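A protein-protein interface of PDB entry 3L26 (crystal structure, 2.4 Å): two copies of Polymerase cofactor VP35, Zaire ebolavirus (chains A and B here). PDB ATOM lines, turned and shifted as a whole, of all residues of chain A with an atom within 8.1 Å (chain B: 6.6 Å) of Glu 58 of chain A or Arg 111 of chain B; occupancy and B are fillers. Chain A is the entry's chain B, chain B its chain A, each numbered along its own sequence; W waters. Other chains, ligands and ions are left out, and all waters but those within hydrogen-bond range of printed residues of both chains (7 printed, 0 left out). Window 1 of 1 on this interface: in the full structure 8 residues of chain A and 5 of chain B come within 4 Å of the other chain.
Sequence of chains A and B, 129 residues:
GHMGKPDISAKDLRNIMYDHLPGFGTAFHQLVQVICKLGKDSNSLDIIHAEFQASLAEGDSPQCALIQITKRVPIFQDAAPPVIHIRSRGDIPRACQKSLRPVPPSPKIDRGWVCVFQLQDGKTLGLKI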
ATOM      1  N   ALA A  50       8.492  -4.847 -18.277  1.00  0.00           N
ATOM      2  CA  ALA A  50       8.447  -4.841 -16.817  1.00  0.00           C
ATOM      3  C   ALA A  50       9.147  -3.599 -16.219  1.00  0.00           C
ATOM      4  O   ALA A  50       8.614  -2.965 -15.299  1.00  0.00           O
ATOM      5  CB  ALA A  50       9.036  -6.142 -16.258  1.00  0.00           C
ATOM      6  N   GLU A  51      10.308  -3.247 -16.772  1.00  0.00           N
ATOM      7  CA  GLU A  51      11.099  -2.088 -16.338  1.00  0.00           C
ATOM      8  C   GLU A  51      10.481  -0.723 -16.691  1.00  0.00           C
ATOM      9  O   GLU A  51      10.557   0.224 -15.906  1.00  0.00           O
ATOM     10  CB  GLU A  51      12.533  -2.190 -16.880  1.00  0.00           C
ATOM     11  CG  GLU A  51      13.471  -1.004 -16.536  1.00  0.00           C
ATOM     12  CD  GLU A  51      13.596  -0.723 -15.037  1.00  0.00           C
ATOM     13  OE1 GLU A  51      13.707  -1.673 -14.228  1.00  0.00           O
ATOM     14  OE2 GLU A  51      13.586   0.463 -14.669  1.00  0.00           O
ATOM     15  N   PHE A  52       9.889  -0.615 -17.872  1.00  0.00           N
ATOM     16  CA  PHE A  52       9.091   0.550 -18.221  1.00  0.00           C
ATOM     17  C   PHE A  52       7.952   0.783 -17.213  1.00  0.00           C
ATOM     18  O   PHE A  52       7.806   1.887 -16.677  1.00  0.00           O
ATOM     19  CB  PHE A  52       8.515   0.369 -19.629  1.00  0.00           C
ATOM     20  CG  PHE A  52       7.833   1.588 -20.173  1.00  0.00           C
ATOM     21  CD1 PHE A  52       8.568   2.745 -20.459  1.00  0.00           C
ATOM     22  CD2 PHE A  52       6.461   1.573 -20.431  1.00  0.00           C
ATOM     23  CE1 PHE A  52       7.952   3.868 -20.971  1.00  0.00           C
ATOM     24  CE2 PHE A  52       5.825   2.705 -20.948  1.00  0.00           C
ATOM     25  CZ  PHE A  52       6.578   3.860 -21.220  1.00  0.00           C
ATOM     26  N   GLN A  53       7.160  -0.254 -16.945  1.00  0.00           N
ATOM     27  CA  GLN A  53       6.000  -0.109 -16.064  1.00  0.00           C
ATOM     28  C   GLN A  53       6.381   0.020 -14.580  1.00  0.00           C
ATOM     29  O   GLN A  53       5.658   0.661 -13.818  1.00  0.00           O
ATOM     30  CB  GLN A  53       4.971  -1.229 -16.306  1.00  0.00           C
ATOM     31  CG  GLN A  53       4.382  -1.264 -17.732  1.00  0.00           C
ATOM     32  CD  GLN A  53       3.205  -0.295 -17.967  1.00  0.00           C
ATOM     33  OE1 GLN A  53       2.735   0.392 -17.054  1.00  0.00           O
ATOM     34  NE2 GLN A  53       2.720  -0.257 -19.205  1.00  0.00           N
ATOM     35  N   ALA A  54       7.512  -0.568 -14.177  1.00  0.00           N
ATOM     36  CA  ALA A  54       8.045  -0.373 -12.813  1.00  0.00           C
ATOM     37  C   ALA A  54       8.540   1.061 -12.546  1.00  0.00           C
ATOM     38  O   ALA A  54       8.328   1.601 -11.453  1.00  0.00           O
ATOM     39  CB  ALA A  54       9.140  -1.394 -12.484  1.00  0.00           C
ATOM     40  N   SER A  55       9.185   1.669 -13.540  1.00  0.00           N
ATOM     41  CA  SER A  55       9.681   3.050 -13.415  1.00  0.00           C
ATOM     42  C   SER A  55       8.554   4.072 -13.383  1.00  0.00           C
ATOM     43  O   SER A  55       8.627   5.039 -12.644  1.00  0.00           O
ATOM     44  CB  SER A  55      10.664   3.378 -14.532  1.00  0.00           C
ATOM     45  OG  SER A  55      11.892   2.719 -14.306  1.00  0.00           O
ATOM     46  N   LEU A  56       7.515   3.844 -14.185  1.00  0.00           N
ATOM     47  CA  LEU A  56       6.314   4.679 -14.167  1.00  0.00           C
ATOM     48  C   LEU A  56       5.610   4.595 -12.825  1.00  0.00           C
ATOM     49  O   LEU A  56       5.118   5.601 -12.315  1.00  0.00           O
ATOM     50  CB  LEU A  56       5.327   4.258 -15.260  1.00  0.00           C
ATOM     51  CG  LEU A  56       5.653   4.487 -16.733  1.00  0.00           C
ATOM     52  CD1 LEU A  56       4.534   3.909 -17.603  1.00  0.00           C
ATOM     53  CD2 LEU A  56       5.902   5.963 -17.032  1.00  0.00           C
ATOM     54  N   ALA A  57       5.561   3.387 -12.264  1.00  0.00           N
ATOM     55  CA  ALA A  57       4.848   3.141 -11.020  1.00  0.00           C
ATOM     56  C   ALA A  57       5.477   3.887  -9.852  1.00  0.00           C
ATOM     57  O   ALA A  57       4.785   4.244  -8.893  1.00  0.00           O
ATOM     58  CB  ALA A  57       4.784   1.657 -10.730  1.00  0.00           C
ATOM     59  N   GLU A  58       6.784   4.119  -9.929  1.00  0.00           N
ATOM     60  CA  GLU A  58       7.465   4.859  -8.877  1.00  0.00           C
ATOM     61  C   GLU A  58       7.630   6.360  -9.185  1.00  0.00           C
ATOM     62  O   GLU A  58       8.357   7.068  -8.475  1.00  0.00           O
ATOM     63  CB  GLU A  58       8.777   4.171  -8.453  1.00  0.00           C
ATOM     64  CG  GLU A  58       9.813   3.980  -9.536  1.00  0.00           C
ATOM     65  CD  GLU A  58      11.015   3.159  -9.062  1.00  0.00           C
ATOM     66  OE1 GLU A  58      11.178   2.956  -7.840  1.00  0.00           O
ATOM     67  OE2 GLU A  58      11.804   2.710  -9.907  1.00  0.00           O
ATOM     68  N   GLY A  59       6.930   6.833 -10.222  1.00  0.00           N
ATOM     69  CA  GLY A  59       6.809   8.262 -10.504  1.00  0.00           C
ATOM     70  C   GLY A  59       7.715   8.850 -11.578  1.00  0.00           C
ATOM     71  O   GLY A  59       7.843  10.075 -11.679  1.00  0.00           O
ATOM     72  N   ASP A  60       8.356   7.998 -12.373  1.00  0.00           N
ATOM     73  CA  ASP A  60       9.135   8.471 -13.519  1.00  0.00           C
ATOM     74  C   ASP A  60       8.217   8.943 -14.655  1.00  0.00           C
ATOM     75  O   ASP A  60       7.156   8.340 -14.912  1.00  0.00           O
ATOM     76  CB  ASP A  60      10.108   7.383 -14.018  1.00  0.00           C
ATOM     77  CG  ASP A  60      11.279   7.153 -13.059  1.00  0.00           C
ATOM     78  OD1 ASP A  60      11.460   7.959 -12.116  1.00  0.00           O
ATOM     79  OD2 ASP A  60      12.020   6.167 -13.247  1.00  0.00           O
ATOM     80  N   SER A  61       8.610  10.038 -15.311  1.00  0.00           N
ATOM     81  CA  SER A  61       7.994  10.434 -16.574  1.00  0.00           C
ATOM     82  C   SER A  61       8.183   9.276 -17.574  1.00  0.00           C
ATOM     83  O   SER A  61       9.047   8.425 -17.358  1.00  0.00           O
ATOM     84  CB  SER A  61       8.641  11.725 -17.101  1.00  0.00           C
ATOM     85  OG  SER A  61      10.010  11.531 -17.460  1.00  0.00           O
ATOM     86  N   ALA A  65      11.483   6.934 -17.927  1.00  0.00           N
ATOM     87  CA  ALA A  65      11.273   5.479 -17.870  1.00  0.00           C
ATOM     88  C   ALA A  65      11.983   4.716 -19.006  1.00  0.00           C
ATOM     89  O   ALA A  65      12.469   3.593 -18.794  1.00  0.00           O
ATOM     90  CB  ALA A  65       9.784   5.155 -17.824  1.00  0.00           C
ATOM     91  N   GLN A  68      15.604   4.742 -18.085  1.00  0.00           N
ATOM     92  CA  GLN A  68      15.780   3.680 -17.078  1.00  0.00           C
ATOM     93  C   GLN A  68      15.953   2.290 -17.683  1.00  0.00           C
ATOM     94  O   GLN A  68      16.623   1.434 -17.105  1.00  0.00           O
ATOM     95  CB  GLN A  68      14.594   3.639 -16.103  1.00  0.00           C
ATOM     96  CG  GLN A  68      14.258   4.937 -15.390  1.00  0.00           C
ATOM     97  CD  GLN A  68      15.383   5.478 -14.531  1.00  0.00           C
ATOM     98  OE1 GLN A  68      16.541   5.071 -14.654  1.00  0.00           O
ATOM     99  NE2 GLN A  68      15.046   6.407 -13.652  1.00  0.00           N
ATOM    100  N   ILE A  69      15.315   2.073 -18.829  1.00  0.00           N
ATOM    101  CA  ILE A  69      15.498   0.855 -19.612  1.00  0.00           C
ATOM    102  C   ILE A  69      16.953   0.717 -20.081  1.00  0.00           C
ATOM    103  O   ILE A  69      17.575  -0.337 -19.900  1.00  0.00           O
ATOM    104  CB  ILE A  69      14.496   0.802 -20.801  1.00  0.00           C
ATOM    105  CG1 ILE A  69      13.134   0.322 -20.297  1.00  0.00           C
ATOM    106  CG2 ILE A  69      15.025  -0.096 -21.935  1.00  0.00           C
ATOM    107  CD1 ILE A  69      11.979   0.935 -21.014  1.00  0.00           C
ATOM    108  N   ARG A  72      19.354  -0.075 -16.976  1.00  0.00           N
ATOM    109  CA  ARG A  72      19.076  -1.218 -16.107  1.00  0.00           C
ATOM    110  C   ARG A  72      18.881  -2.527 -16.858  1.00  0.00           C
ATOM    111  O   ARG A  72      19.177  -3.596 -16.317  1.00  0.00           O
ATOM    112  CB  ARG A  72      17.827  -0.952 -15.259  1.00  0.00           C
ATOM    113  CG  ARG A  72      18.003   0.088 -14.176  1.00  0.00           C
ATOM    114  CD  ARG A  72      16.668   0.581 -13.664  1.00  0.00           C
ATOM    115  NE  ARG A  72      16.847   1.628 -12.663  1.00  0.00           N
ATOM    116  CZ  ARG A  72      15.912   2.490 -12.279  1.00  0.00           C
ATOM    117  NH1 ARG A  72      14.686   2.451 -12.795  1.00  0.00           N
ATOM    118  NH2 ARG A  72      16.211   3.396 -11.363  1.00  0.00           N
ATOM    119  N   VAL A  73      18.352  -2.466 -18.082  1.00  0.00           N
ATOM    120  CA  VAL A  73      18.163  -3.694 -18.860  1.00  0.00           C
ATOM    121  C   VAL A  73      19.495  -4.088 -19.512  1.00  0.00           C
ATOM    122  O   VAL A  73      20.035  -3.324 -20.319  1.00  0.00           O
ATOM    123  CB  VAL A  73      16.993  -3.613 -19.883  1.00  0.00           C
ATOM    124  CG1 VAL A  73      16.895  -4.915 -20.681  1.00  0.00           C
ATOM    125  CG2 VAL A  73      15.679  -3.357 -19.167  1.00  0.00           C
ATOM    126  N   THR B  70      26.155   1.313  -5.258  1.00  0.00           N
ATOM    127  CA  THR B  70      24.787   0.860  -4.929  1.00  0.00           C
ATOM    128  C   THR B  70      24.385  -0.443  -5.636  1.00  0.00           C
ATOM    129  O   THR B  70      23.528  -1.192  -5.140  1.00  0.00           O
ATOM    130  CB  THR B  70      23.687   1.967  -5.164  1.00  0.00           C
ATOM    131  OG1 THR B  70      23.486   2.210  -6.568  1.00  0.00           O
ATOM    132  CG2 THR B  70      24.051   3.269  -4.457  1.00  0.00           C
ATOM    133  N   LYS B  71      25.034  -0.719  -6.768  1.00  0.00           N
ATOM    134  CA  LYS B  71      24.689  -1.854  -7.626  1.00  0.00           C
ATOM    135  C   LYS B  71      25.613  -3.066  -7.469  1.00  0.00           C
ATOM    136  O   LYS B  71      25.257  -4.177  -7.872  1.00  0.00           O
ATOM    137  CB  LYS B  71      24.648  -1.406  -9.092  1.00  0.00           C
ATOM    138  CG  LYS B  71      23.578  -0.368  -9.392  1.00  0.00           C
ATOM    139  CD  LYS B  71      23.424  -0.161 -10.874  1.00  0.00           C
ATOM    140  CE  LYS B  71      22.419   0.927 -11.188  1.00  0.00           C
ATOM    141  NZ  LYS B  71      22.222   1.022 -12.675  1.00  0.00           N
ATOM    142  N   ARG B 101       9.906  12.897  -3.844  1.00  0.00           N
ATOM    143  CA  ARG B 101       8.612  12.369  -4.266  1.00  0.00           C
ATOM    144  C   ARG B 101       7.958  11.482  -3.212  1.00  0.00           C
ATOM    145  O   ARG B 101       8.620  11.073  -2.251  1.00  0.00           O
ATOM    146  CB  ARG B 101       8.697  11.666  -5.632  1.00  0.00           C
ATOM    147  CG  ARG B 101       9.944  10.912  -5.896  1.00  0.00           C
ATOM    148  CD  ARG B 101       9.830  10.139  -7.196  1.00  0.00           C
ATOM    149  NE  ARG B 101      10.493  10.786  -8.329  1.00  0.00           N
ATOM    150  CZ  ARG B 101      10.730  10.169  -9.486  1.00  0.00           C
ATOM    151  NH1 ARG B 101      10.359   8.897  -9.650  1.00  0.00           N
ATOM    152  NH2 ARG B 101      11.340  10.811 -10.475  1.00  0.00           N
ATOM    153  N   PRO B 102       6.646  11.206  -3.367  1.00  0.00           N
ATOM    154  CA  PRO B 102       6.030  10.203  -2.503  1.00  0.00           C
ATOM    155  C   PRO B 102       6.819   8.896  -2.559  1.00  0.00           C
ATOM    156  O   PRO B 102       7.356   8.516  -3.611  1.00  0.00           O
ATOM    157  CB  PRO B 102       4.641  10.005  -3.117  1.00  0.00           C
ATOM    158  CG  PRO B 102       4.349  11.277  -3.825  1.00  0.00           C
ATOM    159  CD  PRO B 102       5.677  11.787  -4.323  1.00  0.00           C
ATOM    160  N   PRO B 104       7.318   5.030  -2.784  1.00  0.00           N
ATOM    161  CA  PRO B 104       6.598   3.895  -3.329  1.00  0.00           C
ATOM    162  C   PRO B 104       6.564   2.769  -2.284  1.00  0.00           C
ATOM    163  O   PRO B 104       7.247   2.866  -1.261  1.00  0.00           O
ATOM    164  CB  PRO B 104       7.456   3.510  -4.546  1.00  0.00           C
ATOM    165  CG  PRO B 104       8.834   3.837  -4.135  1.00  0.00           C
ATOM    166  CD  PRO B 104       8.706   5.083  -3.290  1.00  0.00           C
ATOM    167  N   SER B 106       7.859  -0.258  -2.394  1.00  0.00           N
ATOM    168  CA  SER B 106       9.136  -0.961  -2.254  1.00  0.00           C
ATOM    169  C   SER B 106      10.302  -0.219  -2.896  1.00  0.00           C
ATOM    170  O   SER B 106      10.824  -0.666  -3.928  1.00  0.00           O
ATOM    171  CB  SER B 106       9.037  -2.393  -2.801  1.00  0.00           C
ATOM    172  OG  SER B 106       8.273  -3.218  -1.928  1.00  0.00           O
ATOM    173  N   PRO B 107      10.734   0.901  -2.283  1.00  0.00           N
ATOM    174  CA  PRO B 107      11.845   1.635  -2.885  1.00  0.00           C
ATOM    175  C   PRO B 107      13.178   0.943  -2.599  1.00  0.00           C
ATOM    176  O   PRO B 107      13.338   0.323  -1.538  1.00  0.00           O
ATOM    177  CB  PRO B 107      11.780   3.001  -2.207  1.00  0.00           C
ATOM    178  CG  PRO B 107      11.099   2.757  -0.900  1.00  0.00           C
ATOM    179  CD  PRO B 107      10.262   1.525  -1.030  1.00  0.00           C
ATOM    180  N   LYS B 108      14.104   1.028  -3.555  1.00  0.00           N
ATOM    181  CA  LYS B 108      15.401   0.384  -3.444  1.00  0.00           C
ATOM    182  C   LYS B 108      16.505   1.399  -3.685  1.00  0.00           C
ATOM    183  O   LYS B 108      16.372   2.286  -4.540  1.00  0.00           O
ATOM    184  CB  LYS B 108      15.554  -0.756  -4.462  1.00  0.00           C
ATOM    185  CG  LYS B 108      14.498  -1.833  -4.446  1.00  0.00           C
ATOM    186  CD  LYS B 108      14.413  -2.577  -3.110  1.00  0.00           C
ATOM    187  CE  LYS B 108      13.397  -3.729  -3.192  1.00  0.00           C
ATOM    188  NZ  LYS B 108      12.956  -4.138  -1.815  1.00  0.00           N
ATOM    189  N   ILE B 109      17.601   1.256  -2.940  1.00  0.00           N
ATOM    190  CA  ILE B 109      18.793   2.088  -3.127  1.00  0.00           C
ATOM    191  C   ILE B 109      19.392   1.913  -4.536  1.00  0.00           C
ATOM    192  O   ILE B 109      19.784   2.895  -5.169  1.00  0.00           O
ATOM    193  CB  ILE B 109      19.847   1.824  -2.015  1.00  0.00           C
ATOM    194  CG1 ILE B 109      19.219   2.078  -0.643  1.00  0.00           C
ATOM    195  CG2 ILE B 109      21.080   2.689  -2.212  1.00  0.00           C
ATOM    196  CD1 ILE B 109      20.132   1.801   0.527  1.00  0.00           C
ATOM    197  N   ASP B 110      19.416   0.675  -5.037  1.00  0.00           N
ATOM    198  CA  ASP B 110      19.924   0.389  -6.388  1.00  0.00           C
ATOM    199  C   ASP B 110      18.982   0.829  -7.530  1.00  0.00           C
ATOM    200  O   ASP B 110      19.266   0.597  -8.712  1.00  0.00           O
ATOM    201  CB  ASP B 110      20.364  -1.087  -6.530  1.00  0.00           C
ATOM    202  CG  ASP B 110      19.222  -2.097  -6.337  1.00  0.00           C
ATOM    203  OD1 ASP B 110      18.040  -1.724  -6.235  1.00  0.00           O
ATOM    204  OD2 ASP B 110      19.520  -3.303  -6.294  1.00  0.00           O
ATOM    205  N   ARG B 111      17.868   1.459  -7.167  1.00  0.00           N
ATOM    206  CA  ARG B 111      16.999   2.132  -8.139  1.00  0.00           C
ATOM    207  C   ARG B 111      16.942   3.657  -7.935  1.00  0.00           C
ATOM    208  O   ARG B 111      16.058   4.326  -8.458  1.00  0.00           O
ATOM    209  CB  ARG B 111      15.603   1.520  -8.136  1.00  0.00           C
ATOM    210  CG  ARG B 111      15.547   0.140  -8.763  1.00  0.00           C
ATOM    211  CD  ARG B 111      14.153  -0.463  -8.660  1.00  0.00           C
ATOM    212  NE  ARG B 111      13.243   0.052  -9.686  1.00  0.00           N
ATOM    213  CZ  ARG B 111      13.223  -0.342 -10.961  1.00  0.00           C
ATOM    214  NH1 ARG B 111      14.079  -1.255 -11.405  1.00  0.00           N
ATOM    215  NH2 ARG B 111      12.347   0.189 -11.805  1.00  0.00           N
ATOM    216  N   GLY B 112      17.896   4.187  -7.165  1.00  0.00           N
ATOM    217  CA  GLY B 112      18.034   5.627  -6.964  1.00  0.00           C
ATOM    218  C   GLY B 112      17.262   6.229  -5.801  1.00  0.00           C
ATOM    219  O   GLY B 112      17.219   7.451  -5.680  1.00  0.00           O
ATOM    220  N   TRP B 113      16.639   5.396  -4.961  1.00  0.00           N
ATOM    221  CA  TRP B 113      15.999   5.887  -3.717  1.00  0.00           C
ATOM    222  C   TRP B 113      17.055   6.020  -2.616  1.00  0.00           C
ATOM    223  O   TRP B 113      17.458   5.030  -2.013  1.00  0.00           O
ATOM    224  CB  TRP B 113      14.836   4.992  -3.281  1.00  0.00           C
ATOM    225  CG  TRP B 113      13.715   4.975  -4.291  1.00  0.00           C
ATOM    226  CD1 TRP B 113      13.517   4.050  -5.296  1.00  0.00           C
ATOM    227  CD2 TRP B 113      12.671   5.948  -4.433  1.00  0.00           C
ATOM    228  NE1 TRP B 113      12.402   4.382  -6.032  1.00  0.00           N
ATOM    229  CE2 TRP B 113      11.863   5.542  -5.530  1.00  0.00           C
ATOM    230  CE3 TRP B 113      12.330   7.118  -3.734  1.00  0.00           C
ATOM    231  CZ2 TRP B 113      10.735   6.270  -5.946  1.00  0.00           C
ATOM    232  CZ3 TRP B 113      11.205   7.842  -4.148  1.00  0.00           C
ATOM    233  CH2 TRP B 113      10.421   7.405  -5.244  1.00  0.00           C
ATOM    234  N   LYS B 128      15.056  10.824  -4.561  1.00  0.00           N
ATOM    235  CA  LYS B 128      15.226   9.998  -5.769  1.00  0.00           C
ATOM    236  C   LYS B 128      16.355  10.493  -6.701  1.00  0.00           C
ATOM    237  O   LYS B 128      16.426  11.683  -7.038  1.00  0.00           O
ATOM    238  CB  LYS B 128      13.888   9.903  -6.527  1.00  0.00           C
ATOM    239  CG  LYS B 128      13.851   8.988  -7.773  1.00  0.00           C
ATOM    240  CD  LYS B 128      14.122   7.511  -7.427  1.00  0.00           C
ATOM    241  CE  LYS B 128      13.537   6.576  -8.468  1.00  0.00           C
ATOM    242  NZ  LYS B 128      14.412   6.381  -9.651  1.00  0.00           N
ATOM    243  N   ILE B 129      17.240   9.567  -7.079  1.00  0.00           N
ATOM    244  CA  ILE B 129      18.200   9.760  -8.163  1.00  0.00           C
ATOM    245  C   ILE B 129      17.716   8.999  -9.424  1.00  0.00           C
ATOM    246  O   ILE B 129      17.264   7.849  -9.361  1.00  0.00           O
ATOM    247  CB  ILE B 129      19.651   9.335  -7.750  1.00  0.00           C
ATOM    248  CG1 ILE B 129      20.208  10.295  -6.688  1.00  0.00           C
ATOM    249  CG2 ILE B 129      20.574   9.278  -8.966  1.00  0.00           C
ATOM    250  CD1 ILE B 129      21.610   9.956  -6.164  1.00  0.00           C
ATOM    251  OXT ILE B 129      17.730   9.523 -10.543  1.00  0.00           O
HETATM  252  O   HOH W   1      19.340   2.272 -11.209  1.00  0.00           O
HETATM  253  O   HOH W   2      10.767  11.545 -13.620  1.00  0.00           O
HETATM  254  O   HOH W   3      13.498   4.391 -11.187  1.00  0.00           O
HETATM  255  O   HOH W   4      18.139   5.682 -10.598  1.00  0.00           O
HETATM  256  O   HOH W   5       6.548   8.294  -6.480  1.00  0.00           O
HETATM  257  O   HOH W   6      14.265   8.729 -11.397  1.00  0.00           O
HETATM  258  O   HOH W   7      12.475   0.835  -5.889  1.00  0.00           O
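NH1 of Arg 101 of chain B sits at hydrogen-bond distance from O of Glu 58 of chain A (3.0 Å).
The guanidinium group (NH1) of Arg 101 of chain B lies close to the backbone carbonyl oxygen (O) of Gly 59 of chain A (3.4 Å).
The side-chain carboxylate of Asp 60 of chain A lies within salt-bridge range of the guanidinium group of Arg 101 of chain B (2.9 Å).
The guanidinium group of Arg 111 of chain B lies within salt-bridge range of the side-chain carboxylate of Glu 51 of chain A, 2.9 Å away.
The guanidinium group of Arg 111 of chain B lies within salt-bridge range of the side-chain carboxylate of Glu 58 of chain A, 3.0 Å away.
The guanidinium group of Arg 72 of chain A sits at hydrogen-bond distance from the backbone carbonyl oxygen of Arg 111 of chain B (3.1 Å).
The side-chain carboxylate (OE1) of Glu 58 of chain A sits at hydrogen-bond distance from the indole nitrogen (NE1) of Trp 113 of chain B (2.6 Å).
O of Lys 108 of chain B is in hydrogen-bond range of N of Trp 113 of chain B, 3.1 Å away.
NZ of Lys 128 of chain B lies within hydrogen-bond range of O of Arg 111 of chain B, 2.9 Å away.
OE2 of Glu 51 of chain A lies within hydrogen-bond range of OG of Ser 55 of chain A (2.8 Å).
The guanidinium group (NH1) of Arg 72 of chain A is in salt-bridge range of the side-chain carboxylate (OE2) of Glu 51 of chain A (2.9 Å).
The backbone NH (N) of Asp 60 of chain A is in hydrogen-bond range of the backbone carbonyl oxygen (O) of Ser 55 of chain A (3.0 Å).
The side-chain hydroxyl (OG) of Ser 55 of chain A is in hydrogen-bond range of the guanidinium group (NH1) of Arg 72 of chain A, 3.2 Å away.
Arg 111 of chain B touches Ala 54 of chain A (NH2 to CB, 3.6 Å).
Arg 111 of chain B touches Ser 55 of chain A.
Lys 128 of chain B touches Arg 72 of chain A (NZ to NH2, 3.9 Å).
Printed residues of chain B within 4 Å of Glu 51 of chain A: Arg 111.
Glu 58 of chain A touches three residues of chain B.
Printed residues of chain B within 4 Å of Arg 72 of chain A: Arg 111 and Lys 128.
Of the printed residues of chain A, Arg 101 of chain B touches Glu 58, Gly 59 and Asp 60.
Of the printed residues of chain A, Arg 111 of chain B touches Glu 51, Ala 54, Ser 55, Glu 58 and Arg 72.
The nearest printed residue of chain A that does not touch Arg 101 of chain B is Ser 55 of chain A (5.2 Å).
Hydrophobic or aromatic side chains of chain B within 4 Å of the printed part of chain A: Trp 113.
Of the 17 printed residues of chain A, 7 touch a printed residue of chain B.
Hydrophobic or aromatic side chains of chain A within 4 Å of the printed part of chain B: Ala 54.
No position is printed for both chains.
Water W4 lies within hydrogen-bond range of the chain-end carboxylate of Ile 129 of chain B (2.6 Å), the guanidinium group of Arg 72 of chain A (3.1 Å) and the backbone carbonyl oxygen of Arg 111 of chain B (3.3 Å).
Water W3 lies within hydrogen-bond range of NZ of Lys 128 of chain B (2.7 Å), OE2 of Glu 58 of chain A (2.7 Å), NH1 of Arg 72 of chain A (2.8 Å) and OD2 of Asp 60 of chain A (3.1 Å).
Water W7 lies within hydrogen-bond range of N of Lys 108 of chain B, O of Ser 106 of chain B and OE1 of Glu 58 of chain A.
Water W6 lies within hydrogen-bond range of NZ of Lys 128 of chain B, OD1 of Asp 60 of chain A and NE2 of Gln 68 of chain A.
Water W5 bridges O of Glu 58 of chain A (3.0 Å) and O of Pro 102 of chain B (3.0 Å).
Water W2 lies within hydrogen-bond range of the backbone NH of Ser 61 of chain A and the guanidinium group of Arg 101 of chain B.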
